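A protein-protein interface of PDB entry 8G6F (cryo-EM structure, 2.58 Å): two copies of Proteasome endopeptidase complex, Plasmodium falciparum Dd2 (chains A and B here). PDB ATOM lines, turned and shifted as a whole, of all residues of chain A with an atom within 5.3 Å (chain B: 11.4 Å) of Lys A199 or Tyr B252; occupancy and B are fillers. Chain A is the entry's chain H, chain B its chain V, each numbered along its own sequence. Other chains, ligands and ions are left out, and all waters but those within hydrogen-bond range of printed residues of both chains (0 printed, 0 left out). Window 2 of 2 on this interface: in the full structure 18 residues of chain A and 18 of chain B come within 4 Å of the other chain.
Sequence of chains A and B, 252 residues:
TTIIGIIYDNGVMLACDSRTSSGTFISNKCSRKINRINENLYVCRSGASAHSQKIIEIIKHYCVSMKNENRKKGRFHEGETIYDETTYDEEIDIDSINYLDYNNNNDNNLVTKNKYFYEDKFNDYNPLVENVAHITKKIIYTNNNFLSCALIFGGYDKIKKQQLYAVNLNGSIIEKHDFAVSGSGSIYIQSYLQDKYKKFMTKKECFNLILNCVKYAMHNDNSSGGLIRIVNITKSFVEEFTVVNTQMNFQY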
ATOM      1  N   HIS A 177       3.429  11.690  15.323  1.00  0.00           N
ATOM      2  CA  HIS A 177       2.366  11.889  16.294  1.00  0.00           C
ATOM      3  C   HIS A 177       1.094  11.142  15.940  1.00  0.00           C
ATOM      4  O   HIS A 177       0.176  11.090  16.764  1.00  0.00           O
ATOM      5  CB  HIS A 177       2.064  13.380  16.436  1.00  0.00           C
ATOM      6  CG  HIS A 177       3.213  14.173  16.971  1.00  0.00           C
ATOM      7  ND1 HIS A 177       3.528  14.209  18.311  1.00  0.00           N
ATOM      8  CD2 HIS A 177       4.133  14.943  16.346  1.00  0.00           C
ATOM      9  CE1 HIS A 177       4.589  14.974  18.489  1.00  0.00           C
ATOM     10  NE2 HIS A 177       4.975  15.431  17.313  1.00  0.00           N
ATOM     11  N   ASP A 178       1.010  10.576  14.739  1.00  0.00           N
ATOM     12  CA  ASP A 178      -0.133   9.768  14.337  1.00  0.00           C
ATOM     13  C   ASP A 178       0.266   8.325  14.069  1.00  0.00           C
ATOM     14  O   ASP A 178      -0.267   7.416  14.710  1.00  0.00           O
ATOM     15  CB  ASP A 178      -0.793  10.386  13.098  1.00  0.00           C
ATOM     16  CG  ASP A 178       0.214  10.840  12.067  1.00  0.00           C
ATOM     17  OD1 ASP A 178       1.401  10.487  12.199  1.00  0.00           O
ATOM     18  OD2 ASP A 178      -0.179  11.550  11.120  1.00  0.00           O
ATOM     19  N   PHE A 179       1.204   8.086  13.159  1.00  0.00           N
ATOM     20  CA  PHE A 179       1.595   6.727  12.822  1.00  0.00           C
ATOM     21  C   PHE A 179       2.892   6.763  12.033  1.00  0.00           C
ATOM     22  O   PHE A 179       3.275   7.792  11.475  1.00  0.00           O
ATOM     23  CB  PHE A 179       0.501   6.006  12.027  1.00  0.00           C
ATOM     24  CG  PHE A 179       0.052   6.744  10.803  1.00  0.00           C
ATOM     25  CD1 PHE A 179       0.760   6.650   9.621  1.00  0.00           C
ATOM     26  CD2 PHE A 179      -1.082   7.527  10.831  1.00  0.00           C
ATOM     27  CE1 PHE A 179       0.348   7.328   8.500  1.00  0.00           C
ATOM     28  CE2 PHE A 179      -1.496   8.204   9.710  1.00  0.00           C
ATOM     29  CZ  PHE A 179      -0.783   8.102   8.544  1.00  0.00           C
ATOM     30  N   GLN A 194      -3.624   6.133   5.719  1.00  0.00           N
ATOM     31  CA  GLN A 194      -3.931   7.558   5.745  1.00  0.00           C
ATOM     32  C   GLN A 194      -5.431   7.793   5.741  1.00  0.00           C
ATOM     33  O   GLN A 194      -5.933   8.678   6.441  1.00  0.00           O
ATOM     34  CB  GLN A 194      -3.287   8.249   4.548  1.00  0.00           C
ATOM     35  CG  GLN A 194      -1.860   8.677   4.784  1.00  0.00           C
ATOM     36  CD  GLN A 194      -1.101   9.021   3.513  1.00  0.00           C
ATOM     37  OE1 GLN A 194       0.085   9.326   3.568  1.00  0.00           O
ATOM     38  NE2 GLN A 194      -1.772   8.975   2.369  1.00  0.00           N
ATOM     39  N   TYR A 197      -7.022   6.190   9.334  1.00  0.00           N
ATOM     40  CA  TYR A 197      -6.579   6.661  10.637  1.00  0.00           C
ATOM     41  C   TYR A 197      -7.432   7.830  11.117  1.00  0.00           C
ATOM     42  O   TYR A 197      -7.887   8.663  10.332  1.00  0.00           O
ATOM     43  CB  TYR A 197      -5.113   7.080  10.579  1.00  0.00           C
ATOM     44  CG  TYR A 197      -4.588   7.624  11.884  1.00  0.00           C
ATOM     45  CD1 TYR A 197      -4.214   6.774  12.912  1.00  0.00           C
ATOM     46  CD2 TYR A 197      -4.469   8.988  12.089  1.00  0.00           C
ATOM     47  CE1 TYR A 197      -3.738   7.268  14.101  1.00  0.00           C
ATOM     48  CE2 TYR A 197      -3.998   9.488  13.272  1.00  0.00           C
ATOM     49  CZ  TYR A 197      -3.632   8.625  14.276  1.00  0.00           C
ATOM     50  OH  TYR A 197      -3.160   9.126  15.461  1.00  0.00           O
ATOM     51  N   LYS A 198      -7.644   7.882  12.430  1.00  0.00           N
ATOM     52  CA  LYS A 198      -8.308   9.011  13.066  1.00  0.00           C
ATOM     53  C   LYS A 198      -7.691   9.220  14.439  1.00  0.00           C
ATOM     54  O   LYS A 198      -7.041   8.330  14.989  1.00  0.00           O
ATOM     55  CB  LYS A 198      -9.821   8.795  13.170  1.00  0.00           C
ATOM     56  CG  LYS A 198     -10.260   7.950  14.345  1.00  0.00           C
ATOM     57  CD  LYS A 198     -11.762   7.757  14.358  1.00  0.00           C
ATOM     58  CE  LYS A 198     -12.179   6.572  13.509  1.00  0.00           C
ATOM     59  NZ  LYS A 198     -11.821   5.277  14.141  1.00  0.00           N
ATOM     60  N   LYS A 199      -7.893  10.416  14.984  1.00  0.00           N
ATOM     61  CA  LYS A 199      -7.323  10.768  16.277  1.00  0.00           C
ATOM     62  C   LYS A 199      -8.142  10.180  17.419  1.00  0.00           C
ATOM     63  O   LYS A 199      -9.374  10.155  17.373  1.00  0.00           O
ATOM     64  CB  LYS A 199      -7.249  12.284  16.428  1.00  0.00           C
ATOM     65  CG  LYS A 199      -6.156  12.935  15.617  1.00  0.00           C
ATOM     66  CD  LYS A 199      -6.051  14.418  15.929  1.00  0.00           C
ATOM     67  CE  LYS A 199      -4.963  14.698  16.953  1.00  0.00           C
ATOM     68  NZ  LYS A 199      -3.599  14.567  16.372  1.00  0.00           N
ATOM     69  N   PHE A 200      -7.442   9.721  18.456  1.00  0.00           N
ATOM     70  CA  PHE A 200      -8.068   9.166  19.656  1.00  0.00           C
ATOM     71  C   PHE A 200      -8.906   7.933  19.324  1.00  0.00           C
ATOM     72  O   PHE A 200     -10.067   7.819  19.717  1.00  0.00           O
ATOM     73  CB  PHE A 200      -8.919  10.214  20.373  1.00  0.00           C
ATOM     74  CG  PHE A 200      -8.236  11.535  20.547  1.00  0.00           C
ATOM     75  CD1 PHE A 200      -6.984  11.612  21.124  1.00  0.00           C
ATOM     76  CD2 PHE A 200      -8.853  12.703  20.138  1.00  0.00           C
ATOM     77  CE1 PHE A 200      -6.357  12.829  21.283  1.00  0.00           C
ATOM     78  CE2 PHE A 200      -8.229  13.921  20.295  1.00  0.00           C
ATOM     79  CZ  PHE A 200      -6.981  13.983  20.868  1.00  0.00           C
ATOM     80  N   MET A 201      -8.303   6.999  18.599  1.00  0.00           N
ATOM     81  CA  MET A 201      -8.952   5.724  18.353  1.00  0.00           C
ATOM     82  C   MET A 201      -8.988   4.900  19.631  1.00  0.00           C
ATOM     83  O   MET A 201      -8.132   5.035  20.507  1.00  0.00           O
ATOM     84  CB  MET A 201      -8.217   4.952  17.263  1.00  0.00           C
ATOM     85  CG  MET A 201      -8.562   5.394  15.860  1.00  0.00           C
ATOM     86  SD  MET A 201      -7.860   4.355  14.569  1.00  0.00           S
ATOM     87  CE  MET A 201      -6.198   4.127  15.174  1.00  0.00           C
ATOM     88  N   TYR B 192      -5.744   0.532  -0.786  1.00  0.00           N
ATOM     89  CA  TYR B 192      -6.924   1.378  -0.665  1.00  0.00           C
ATOM     90  C   TYR B 192      -7.991   0.970  -1.673  1.00  0.00           C
ATOM     91  O   TYR B 192      -9.164   0.785  -1.321  1.00  0.00           O
ATOM     92  CB  TYR B 192      -6.509   2.835  -0.861  1.00  0.00           C
ATOM     93  CG  TYR B 192      -7.643   3.818  -0.919  1.00  0.00           C
ATOM     94  CD1 TYR B 192      -8.124   4.412   0.231  1.00  0.00           C
ATOM     95  CD2 TYR B 192      -8.224   4.166  -2.127  1.00  0.00           C
ATOM     96  CE1 TYR B 192      -9.155   5.313   0.183  1.00  0.00           C
ATOM     97  CE2 TYR B 192      -9.254   5.066  -2.182  1.00  0.00           C
ATOM     98  CZ  TYR B 192      -9.715   5.638  -1.024  1.00  0.00           C
ATOM     99  OH  TYR B 192     -10.745   6.541  -1.069  1.00  0.00           O
ATOM    100  N   TYR B 216      -5.170  10.324  -3.683  1.00  0.00           N
ATOM    101  CA  TYR B 216      -4.218   9.732  -2.748  1.00  0.00           C
ATOM    102  C   TYR B 216      -2.883   9.451  -3.422  1.00  0.00           C
ATOM    103  O   TYR B 216      -1.816   9.698  -2.838  1.00  0.00           O
ATOM    104  CB  TYR B 216      -4.801   8.452  -2.158  1.00  0.00           C
ATOM    105  CG  TYR B 216      -5.633   8.688  -0.924  1.00  0.00           C
ATOM    106  CD1 TYR B 216      -5.040   9.047   0.275  1.00  0.00           C
ATOM    107  CD2 TYR B 216      -7.010   8.562  -0.959  1.00  0.00           C
ATOM    108  CE1 TYR B 216      -5.793   9.268   1.400  1.00  0.00           C
ATOM    109  CE2 TYR B 216      -7.771   8.782   0.160  1.00  0.00           C
ATOM    110  CZ  TYR B 216      -7.159   9.134   1.339  1.00  0.00           C
ATOM    111  OH  TYR B 216      -7.916   9.356   2.463  1.00  0.00           O
ATOM    112  N   HIS B 219      -1.091  12.660  -3.706  1.00  0.00           N
ATOM    113  CA  HIS B 219      -0.618  13.118  -2.407  1.00  0.00           C
ATOM    114  C   HIS B 219       0.676  12.422  -2.020  1.00  0.00           C
ATOM    115  O   HIS B 219       1.587  13.050  -1.471  1.00  0.00           O
ATOM    116  CB  HIS B 219      -1.685  12.877  -1.341  1.00  0.00           C
ATOM    117  CG  HIS B 219      -1.223  13.176   0.049  1.00  0.00           C
ATOM    118  ND1 HIS B 219      -1.138  14.458   0.543  1.00  0.00           N
ATOM    119  CD2 HIS B 219      -0.815  12.360   1.048  1.00  0.00           C
ATOM    120  CE1 HIS B 219      -0.695  14.420   1.786  1.00  0.00           C
ATOM    121  NE2 HIS B 219      -0.492  13.158   2.116  1.00  0.00           N
ATOM    122  N   ASN B 220       0.777  11.124  -2.292  1.00  0.00           N
ATOM    123  CA  ASN B 220       1.915  10.355  -1.806  1.00  0.00           C
ATOM    124  C   ASN B 220       3.077  10.275  -2.787  1.00  0.00           C
ATOM    125  O   ASN B 220       4.195   9.963  -2.365  1.00  0.00           O
ATOM    126  CB  ASN B 220       1.472   8.936  -1.453  1.00  0.00           C
ATOM    127  CG  ASN B 220       0.677   8.882  -0.176  1.00  0.00           C
ATOM    128  OD1 ASN B 220      -0.501   8.539  -0.182  1.00  0.00           O
ATOM    129  ND2 ASN B 220       1.316   9.226   0.930  1.00  0.00           N
ATOM    130  N   MET B 248      -5.513  17.234  -0.777  1.00  0.00           N
ATOM    131  CA  MET B 248      -5.918  16.224   0.191  1.00  0.00           C
ATOM    132  C   MET B 248      -5.953  16.859   1.574  1.00  0.00           C
ATOM    133  O   MET B 248      -4.936  17.376   2.048  1.00  0.00           O
ATOM    134  CB  MET B 248      -4.952  15.041   0.163  1.00  0.00           C
ATOM    135  CG  MET B 248      -5.569  13.713   0.539  1.00  0.00           C
ATOM    136  SD  MET B 248      -6.195  12.806  -0.879  1.00  0.00           S
ATOM    137  CE  MET B 248      -7.943  12.765  -0.502  1.00  0.00           C
ATOM    138  N   ASN B 249      -7.116  16.821   2.216  1.00  0.00           N
ATOM    139  CA  ASN B 249      -7.315  17.417   3.531  1.00  0.00           C
ATOM    140  C   ASN B 249      -7.567  16.310   4.543  1.00  0.00           C
ATOM    141  O   ASN B 249      -8.501  15.517   4.380  1.00  0.00           O
ATOM    142  CB  ASN B 249      -8.486  18.401   3.511  1.00  0.00           C
ATOM    143  CG  ASN B 249      -8.053  19.833   3.762  1.00  0.00           C
ATOM    144  OD1 ASN B 249      -6.864  20.147   3.774  1.00  0.00           O
ATOM    145  ND2 ASN B 249      -9.026  20.714   3.962  1.00  0.00           N
ATOM    146  N   PHE B 250      -6.743  16.264   5.583  1.00  0.00           N
ATOM    147  CA  PHE B 250      -6.854  15.271   6.640  1.00  0.00           C
ATOM    148  C   PHE B 250      -7.261  15.956   7.937  1.00  0.00           C
ATOM    149  O   PHE B 250      -6.704  16.996   8.301  1.00  0.00           O
ATOM    150  CB  PHE B 250      -5.533  14.527   6.837  1.00  0.00           C
ATOM    151  CG  PHE B 250      -5.126  13.695   5.658  1.00  0.00           C
ATOM    152  CD1 PHE B 250      -5.846  12.569   5.306  1.00  0.00           C
ATOM    153  CD2 PHE B 250      -4.021  14.038   4.900  1.00  0.00           C
ATOM    154  CE1 PHE B 250      -5.474  11.807   4.223  1.00  0.00           C
ATOM    155  CE2 PHE B 250      -3.645  13.273   3.815  1.00  0.00           C
ATOM    156  CZ  PHE B 250      -4.372  12.158   3.478  1.00  0.00           C
ATOM    157  N   GLN B 251      -8.243  15.376   8.627  1.00  0.00           N
ATOM    158  CA  GLN B 251      -8.674  15.943   9.899  1.00  0.00           C
ATOM    159  C   GLN B 251      -7.561  15.868  10.936  1.00  0.00           C
ATOM    160  O   GLN B 251      -7.311  16.835  11.664  1.00  0.00           O
ATOM    161  CB  GLN B 251      -9.925  15.222  10.401  1.00  0.00           C
ATOM    162  CG  GLN B 251     -11.168  15.434   9.547  1.00  0.00           C
ATOM    163  CD  GLN B 251     -11.313  16.863   9.061  1.00  0.00           C
ATOM    164  OE1 GLN B 251     -11.051  17.163   7.896  1.00  0.00           O
ATOM    165  NE2 GLN B 251     -11.731  17.754   9.953  1.00  0.00           N
ATOM    166  N   TYR B 252      -6.874  14.735  11.009  1.00  0.00           N
ATOM    167  CA  TYR B 252      -5.826  14.543  12.000  1.00  0.00           C
ATOM    168  C   TYR B 252      -4.598  15.375  11.661  1.00  0.00           C
ATOM    169  O   TYR B 252      -3.549  15.231  12.286  1.00  0.00           O
ATOM    170  CB  TYR B 252      -5.450  13.062  12.100  1.00  0.00           C
ATOM    171  CG  TYR B 252      -4.813  12.491  10.854  1.00  0.00           C
ATOM    172  CD1 TYR B 252      -3.452  12.620  10.625  1.00  0.00           C
ATOM    173  CD2 TYR B 252      -5.571  11.811   9.914  1.00  0.00           C
ATOM    174  CE1 TYR B 252      -2.867  12.098   9.496  1.00  0.00           C
ATOM    175  CE2 TYR B 252      -4.992  11.282   8.781  1.00  0.00           C
ATOM    176  CZ  TYR B 252      -3.641  11.429   8.579  1.00  0.00           C
ATOM    177  OH  TYR B 252      -3.058  10.909   7.450  1.00  0.00           O
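Hydrophobic or aromatic side chains of chain B that line the printed part of chain A: Tyr B216, His B219, Phe B250 and Tyr B252.
Printed residues of chain A that touch a printed residue of chain B: Asp A178, Phe A179, Gln A194, Tyr A197 and Lys A199.
Among the printed residues, 9 pairs touch across the chains.
Lys A199 touches just one residue of chain B: Tyr B252.
Tyr B252 touches just these residues of chain A: Asp A178, Phe A179, Gln A194, Tyr A197 and Lys A199.
Of the printed residues of chain B, Asp A178 touches Tyr B252 (3.2 Å).
Of the printed residues of chain B, Tyr A197 touches Tyr B252 (3.7 Å).
No residue of chain B comes within 4 Å of Lys A198.
No residue of chain B comes within 4 Å of Phe A200.
Met A201 touches none of the printed residues of chain B.
Of the printed residues of chain A, His B219 touches Gln A194 (3.8 Å).
Of the printed residues of chain A, Phe B250 touches Gln A194.
Printed residues of chain A within 4 Å of Asn B220: Gln A194.
Printed residues of chain A within 4 Å of Tyr B216: Gln A194.
Asn B249 touches none of the printed residues of chain A.
The nearest residue of chain B that does not touch Lys A199 is Gln B251 (5.1 Å).
The nearest residue of chain A that does not touch Tyr B252 is Lys A198 (5.0 Å).
OD1 of Asn B220 sits at hydrogen-bond distance from NE2 of Gln A194 (2.9 Å).
No position is printed for both chains.
Among the printed residues, merely in contact across the chains: Asp A178 with Tyr B252, Phe A179 with Tyr B252, Gln A194 with Tyr B216, Gln A194 with His B219, Gln A194 with Phe B250, Gln A194 with Tyr B252, Tyr A197 with Tyr B252 and Lys A199 with Tyr B252.
The side-chain hydroxyl (OH) of Tyr A197 sits close to the backbone carbonyl oxygen (O) of Asp A178 (3.4 Å).
The backbone carbonyl oxygen (O) of Tyr B216 lies close to the side-chain amide oxygen (OD1) of Asn B220, at 3.2 Å.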
